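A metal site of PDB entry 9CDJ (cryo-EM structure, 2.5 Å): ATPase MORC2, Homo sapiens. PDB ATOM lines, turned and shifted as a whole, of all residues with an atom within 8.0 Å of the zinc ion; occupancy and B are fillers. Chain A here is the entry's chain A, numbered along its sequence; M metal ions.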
ATOM      1  N   GLN A 498     -13.826   1.983 -19.203  1.00  0.00           N
ATOM      2  CA  GLN A 498     -13.088   3.196 -19.512  1.00  0.00           C
ATOM      3  C   GLN A 498     -12.133   3.518 -18.368  1.00  0.00           C
ATOM      4  O   GLN A 498     -12.522   3.513 -17.203  1.00  0.00           O
ATOM      5  CB  GLN A 498     -14.042   4.373 -19.732  1.00  0.00           C
ATOM      6  CG  GLN A 498     -13.339   5.665 -20.109  1.00  0.00           C
ATOM      7  CD  GLN A 498     -14.316   6.789 -20.433  1.00  0.00           C
ATOM      8  OE1 GLN A 498     -15.350   6.929 -19.789  1.00  0.00           O
ATOM      9  NE2 GLN A 498     -13.983   7.592 -21.433  1.00  0.00           N
ATOM     10  N   CYS A 499     -10.876   3.779 -18.723  1.00  0.00           N
ATOM     11  CA  CYS A 499      -9.910   4.217 -17.722  1.00  0.00           C
ATOM     12  C   CYS A 499     -10.260   5.628 -17.265  1.00  0.00           C
ATOM     13  O   CYS A 499     -10.486   6.516 -18.082  1.00  0.00           O
ATOM     14  CB  CYS A 499      -8.494   4.185 -18.298  1.00  0.00           C
ATOM     15  SG  CYS A 499      -7.257   5.027 -17.294  1.00  0.00           S
ATOM     16  N   ASP A 500     -10.292   5.823 -15.948  1.00  0.00           N
ATOM     17  CA  ASP A 500     -10.653   7.107 -15.369  1.00  0.00           C
ATOM     18  C   ASP A 500      -9.533   8.139 -15.451  1.00  0.00           C
ATOM     19  O   ASP A 500      -9.685   9.236 -14.915  1.00  0.00           O
ATOM     20  CB  ASP A 500     -11.086   6.929 -13.914  1.00  0.00           C
ATOM     21  CG  ASP A 500     -12.181   7.882 -13.502  1.00  0.00           C
ATOM     22  OD1 ASP A 500     -11.879   9.071 -13.241  1.00  0.00           O
ATOM     23  OD2 ASP A 500     -13.351   7.461 -13.432  1.00  0.00           O
ATOM     24  N   LEU A 501      -8.419   7.801 -16.088  1.00  0.00           N
ATOM     25  CA  LEU A 501      -7.276   8.699 -16.214  1.00  0.00           C
ATOM     26  C   LEU A 501      -7.025   9.131 -17.644  1.00  0.00           C
ATOM     27  O   LEU A 501      -6.897  10.334 -17.917  1.00  0.00           O
ATOM     28  CB  LEU A 501      -6.022   8.022 -15.636  1.00  0.00           C
ATOM     29  CG  LEU A 501      -5.040   8.950 -14.917  1.00  0.00           C
ATOM     30  CD1 LEU A 501      -4.072   8.142 -14.066  1.00  0.00           C
ATOM     31  CD2 LEU A 501      -4.289   9.820 -15.904  1.00  0.00           C
ATOM     32  N   CYS A 502      -6.949   8.179 -18.580  1.00  0.00           N
ATOM     33  CA  CYS A 502      -6.742   8.498 -19.983  1.00  0.00           C
ATOM     34  C   CYS A 502      -8.035   8.465 -20.803  1.00  0.00           C
ATOM     35  O   CYS A 502      -8.000   8.796 -21.991  1.00  0.00           O
ATOM     36  CB  CYS A 502      -5.740   7.521 -20.601  1.00  0.00           C
ATOM     37  SG  CYS A 502      -6.177   5.771 -20.403  1.00  0.00           S
ATOM     38  N   LEU A 503      -9.154   8.074 -20.200  1.00  0.00           N
ATOM     39  CA  LEU A 503     -10.454   8.029 -20.869  1.00  0.00           C
ATOM     40  C   LEU A 503     -10.466   7.051 -22.041  1.00  0.00           C
ATOM     41  O   LEU A 503     -11.378   7.087 -22.874  1.00  0.00           O
ATOM     42  CB  LEU A 503     -10.878   9.431 -21.345  1.00  0.00           C
ATOM     43  CG  LEU A 503     -11.691  10.246 -20.339  1.00  0.00           C
ATOM     44  CD1 LEU A 503     -10.995  10.270 -18.985  1.00  0.00           C
ATOM     45  CD2 LEU A 503     -11.913  11.652 -20.855  1.00  0.00           C
ATOM     46  N   LYS A 504      -9.478   6.168 -22.117  1.00  0.00           N
ATOM     47  CA  LYS A 504      -9.416   5.172 -23.186  1.00  0.00           C
ATOM     48  C   LYS A 504     -10.269   3.975 -22.804  1.00  0.00           C
ATOM     49  O   LYS A 504     -10.234   3.515 -21.664  1.00  0.00           O
ATOM     50  CB  LYS A 504      -7.976   4.752 -23.446  1.00  0.00           C
ATOM     51  CG  LYS A 504      -7.131   5.832 -24.099  1.00  0.00           C
ATOM     52  CD  LYS A 504      -5.663   5.470 -24.143  1.00  0.00           C
ATOM     53  CE  LYS A 504      -4.815   6.660 -24.576  1.00  0.00           C
ATOM     54  NZ  LYS A 504      -3.372   6.299 -24.725  1.00  0.00           N
ATOM     55  N   TRP A 505     -11.029   3.464 -23.772  1.00  0.00           N
ATOM     56  CA  TRP A 505     -11.957   2.360 -23.516  1.00  0.00           C
ATOM     57  C   TRP A 505     -11.218   1.037 -23.670  1.00  0.00           C
ATOM     58  O   TRP A 505     -10.873   0.642 -24.781  1.00  0.00           O
ATOM     59  CB  TRP A 505     -13.154   2.446 -24.465  1.00  0.00           C
ATOM     60  CG  TRP A 505     -14.294   3.219 -23.905  1.00  0.00           C
ATOM     61  CD1 TRP A 505     -14.657   4.499 -24.227  1.00  0.00           C
ATOM     62  CD2 TRP A 505     -15.216   2.780 -22.905  1.00  0.00           C
ATOM     63  NE1 TRP A 505     -15.754   4.871 -23.487  1.00  0.00           N
ATOM     64  CE2 TRP A 505     -16.118   3.829 -22.678  1.00  0.00           C
ATOM     65  CE3 TRP A 505     -15.369   1.593 -22.190  1.00  0.00           C
ATOM     66  CZ2 TRP A 505     -17.151   3.738 -21.754  1.00  0.00           C
ATOM     67  CZ3 TRP A 505     -16.401   1.502 -21.277  1.00  0.00           C
ATOM     68  CH2 TRP A 505     -17.273   2.563 -21.066  1.00  0.00           C
ATOM     69  N   ARG A 506     -10.987   0.361 -22.554  1.00  0.00           N
ATOM     70  CA  ARG A 506     -10.303  -0.916 -22.546  1.00  0.00           C
ATOM     71  C   ARG A 506     -11.310  -2.061 -22.473  1.00  0.00           C
ATOM     72  O   ARG A 506     -12.471  -1.880 -22.083  1.00  0.00           O
ATOM     73  CB  ARG A 506      -9.326  -0.996 -21.357  1.00  0.00           C
ATOM     74  CG  ARG A 506      -8.338   0.152 -21.302  1.00  0.00           C
ATOM     75  CD  ARG A 506      -7.421   0.143 -22.514  1.00  0.00           C
ATOM     76  NE  ARG A 506      -6.330   1.105 -22.377  1.00  0.00           N
ATOM     77  CZ  ARG A 506      -5.538   1.483 -23.365  1.00  0.00           C
ATOM     78  NH1 ARG A 506      -5.676   1.006 -24.590  1.00  0.00           N
ATOM     79  NH2 ARG A 506      -4.568   2.366 -23.123  1.00  0.00           N
ATOM     80  N   TRP A 523     -11.545   2.290 -11.794  1.00  0.00           N
ATOM     81  CA  TRP A 523     -10.692   1.455 -12.631  1.00  0.00           C
ATOM     82  C   TRP A 523      -9.888   2.296 -13.610  1.00  0.00           C
ATOM     83  O   TRP A 523     -10.383   3.269 -14.178  1.00  0.00           O
ATOM     84  CB  TRP A 523     -11.547   0.442 -13.389  1.00  0.00           C
ATOM     85  CG  TRP A 523     -10.749  -0.577 -14.159  1.00  0.00           C
ATOM     86  CD1 TRP A 523     -10.490  -1.854 -13.783  1.00  0.00           C
ATOM     87  CD2 TRP A 523     -10.137  -0.392 -15.445  1.00  0.00           C
ATOM     88  NE1 TRP A 523      -9.735  -2.481 -14.752  1.00  0.00           N
ATOM     89  CE2 TRP A 523      -9.501  -1.600 -15.770  1.00  0.00           C
ATOM     90  CE3 TRP A 523     -10.049   0.685 -16.329  1.00  0.00           C
ATOM     91  CZ2 TRP A 523      -8.797  -1.778 -16.961  1.00  0.00           C
ATOM     92  CZ3 TRP A 523      -9.347   0.507 -17.510  1.00  0.00           C
ATOM     93  CH2 TRP A 523      -8.727  -0.707 -17.818  1.00  0.00           C
ATOM     94  N   VAL A 524      -8.624   1.914 -13.826  1.00  0.00           N
ATOM     95  CA  VAL A 524      -7.738   2.576 -14.777  1.00  0.00           C
ATOM     96  C   VAL A 524      -6.987   1.511 -15.554  1.00  0.00           C
ATOM     97  O   VAL A 524      -7.019   0.326 -15.236  1.00  0.00           O
ATOM     98  CB  VAL A 524      -6.745   3.545 -14.098  1.00  0.00           C
ATOM     99  CG1 VAL A 524      -7.492   4.741 -13.517  1.00  0.00           C
ATOM    100  CG2 VAL A 524      -5.953   2.833 -13.014  1.00  0.00           C
ATOM    101  N   CYS A 525      -6.298   1.959 -16.611  1.00  0.00           N
ATOM    102  CA  CYS A 525      -5.578   1.035 -17.487  1.00  0.00           C
ATOM    103  C   CYS A 525      -4.593   0.181 -16.704  1.00  0.00           C
ATOM    104  O   CYS A 525      -4.435  -1.011 -16.963  1.00  0.00           O
ATOM    105  CB  CYS A 525      -4.865   1.804 -18.589  1.00  0.00           C
ATOM    106  SG  CYS A 525      -5.960   2.531 -19.823  1.00  0.00           S
ATOM    107  N   SER A 526      -3.910   0.782 -15.720  1.00  0.00           N
ATOM    108  CA  SER A 526      -2.883   0.062 -14.973  1.00  0.00           C
ATOM    109  C   SER A 526      -3.434  -1.185 -14.310  1.00  0.00           C
ATOM    110  O   SER A 526      -2.707  -2.165 -14.121  1.00  0.00           O
ATOM    111  CB  SER A 526      -2.266   0.991 -13.928  1.00  0.00           C
ATOM    112  OG  SER A 526      -1.571   2.060 -14.544  1.00  0.00           O
ATOM    113  N   MET A 527      -4.718  -1.183 -13.945  1.00  0.00           N
ATOM    114  CA  MET A 527      -5.345  -2.318 -13.296  1.00  0.00           C
ATOM    115  C   MET A 527      -5.895  -3.337 -14.289  1.00  0.00           C
ATOM    116  O   MET A 527      -6.604  -4.267 -13.881  1.00  0.00           O
ATOM    117  CB  MET A 527      -6.479  -1.866 -12.362  1.00  0.00           C
ATOM    118  CG  MET A 527      -6.268  -0.486 -11.725  1.00  0.00           C
ATOM    119  SD  MET A 527      -7.741   0.163 -10.910  1.00  0.00           S
ATOM    120  CE  MET A 527      -8.533  -1.338 -10.308  1.00  0.00           C
ATOM    121  N   GLN A 533      -2.669  -4.132 -22.865  1.00  0.00           N
ATOM    122  CA  GLN A 533      -3.351  -2.862 -22.650  1.00  0.00           C
ATOM    123  C   GLN A 533      -3.399  -2.540 -21.156  1.00  0.00           C
ATOM    124  O   GLN A 533      -4.431  -2.165 -20.609  1.00  0.00           O
ATOM    125  CB  GLN A 533      -4.742  -2.888 -23.252  1.00  0.00           C
ATOM    126  CG  GLN A 533      -5.598  -4.045 -22.761  1.00  0.00           C
ATOM    127  CD  GLN A 533      -6.955  -4.102 -23.439  1.00  0.00           C
ATOM    128  OE1 GLN A 533      -7.270  -3.268 -24.289  1.00  0.00           O
ATOM    129  NE2 GLN A 533      -7.761  -5.083 -23.065  1.00  0.00           N
ATOM    130  N   ASP A 534      -2.257  -2.694 -20.477  1.00  0.00           N
ATOM    131  CA  ASP A 534      -2.128  -2.368 -19.067  1.00  0.00           C
ATOM    132  C   ASP A 534      -1.531  -0.972 -18.846  1.00  0.00           C
ATOM    133  O   ASP A 534      -1.051  -0.675 -17.745  1.00  0.00           O
ATOM    134  CB  ASP A 534      -1.324  -3.464 -18.357  1.00  0.00           C
ATOM    135  CG  ASP A 534       0.198  -3.222 -18.346  1.00  0.00           C
ATOM    136  OD1 ASP A 534       0.916  -4.163 -17.946  1.00  0.00           O
ATOM    137  OD2 ASP A 534       0.689  -2.152 -18.761  1.00  0.00           O
ATOM    138  N   ARG A 535      -1.596  -0.114 -19.860  1.00  0.00           N
ATOM    139  CA  ARG A 535      -0.988   1.209 -19.798  1.00  0.00           C
ATOM    140  C   ARG A 535      -1.989   2.240 -20.305  1.00  0.00           C
ATOM    141  O   ARG A 535      -2.875   1.938 -21.105  1.00  0.00           O
ATOM    142  CB  ARG A 535       0.292   1.275 -20.641  1.00  0.00           C
ATOM    143  CG  ARG A 535       1.384   0.319 -20.202  1.00  0.00           C
ATOM    144  CD  ARG A 535       2.759   0.816 -20.636  1.00  0.00           C
ATOM    145  NE  ARG A 535       2.858   1.058 -22.075  1.00  0.00           N
ATOM    146  CZ  ARG A 535       2.552   0.197 -23.033  1.00  0.00           C
ATOM    147  NH1 ARG A 535       2.231  -1.066 -22.758  1.00  0.00           N
ATOM    148  NH2 ARG A 535       2.577   0.586 -24.295  1.00  0.00           N
ATOM    149  N   CYS A 536      -1.827   3.472 -19.814  1.00  0.00           N
ATOM    150  CA  CYS A 536      -2.604   4.585 -20.328  1.00  0.00           C
ATOM    151  C   CYS A 536      -2.083   5.100 -21.657  1.00  0.00           C
ATOM    152  O   CYS A 536      -2.789   5.854 -22.333  1.00  0.00           O
ATOM    153  CB  CYS A 536      -2.618   5.725 -19.306  1.00  0.00           C
ATOM    154  SG  CYS A 536      -3.492   5.338 -17.773  1.00  0.00           S
ATOM    155  N   GLU A 537      -0.864   4.719 -22.053  1.00  0.00           N
ATOM    156  CA  GLU A 537      -0.313   5.095 -23.343  1.00  0.00           C
ATOM    157  C   GLU A 537      -0.615   4.067 -24.428  1.00  0.00           C
ATOM    158  O   GLU A 537      -0.519   4.387 -25.615  1.00  0.00           O
ATOM    159  CB  GLU A 537       1.198   5.285 -23.241  1.00  0.00           C
ATOM    160  CG  GLU A 537       1.631   6.343 -22.238  1.00  0.00           C
ATOM    161  CD  GLU A 537       1.623   5.837 -20.809  1.00  0.00           C
ATOM    162  OE1 GLU A 537       1.457   4.617 -20.602  1.00  0.00           O
ATOM    163  OE2 GLU A 537       1.783   6.665 -19.883  1.00  0.00           O
ATOM    164  N   ALA A 538      -0.981   2.848 -24.040  1.00  0.00           N
ATOM    165  CA  ALA A 538      -1.296   1.810 -25.005  1.00  0.00           C
ATOM    166  C   ALA A 538      -2.422   2.263 -25.922  1.00  0.00           C
ATOM    167  O   ALA A 538      -3.416   2.819 -25.475  1.00  0.00           O
ATOM    168  CB  ALA A 538      -1.679   0.514 -24.294  1.00  0.00           C
HETATM  169 ZN    ZN M   1      -5.488   4.450 -18.642  1.00  0.00          ZN
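N of Leu 501 sits close to SG of Cys 499 (3.2 Å).
N of Cys 499 lies within hydrogen-bond range of O of Lys 504, 3.0 Å away.
The side-chain sulfur (SG) of Cys 525 lies close to the backbone carbonyl oxygen (O) of Arg 535.
NE of Arg 506 sits close to SG of Cys 525 (2.9 Å).
SG of Cys 502 lies close to N of Lys 504 (3.7 Å).
The backbone carbonyl oxygen of Cys 536 is in hydrogen-bond range of the side-chain amino group of Lys 504, 2.5 Å away.
Within 4 Å of the zinc ion: Cys 499, Cys 502, Cys 525 and Cys 536.
Along chain A the residues within 4 Å of the zinc ion span positions 499 to 536.
The zinc ion is bound by the side-chain sulfur (SG) of Cys 499 (2.3 Å), the side-chain sulfur (SG) of Cys 525 (2.3 Å), the side-chain sulfur (SG) of Cys 502 (2.3 Å) and the side-chain sulfur (SG) of Cys 536 (2.4 Å).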
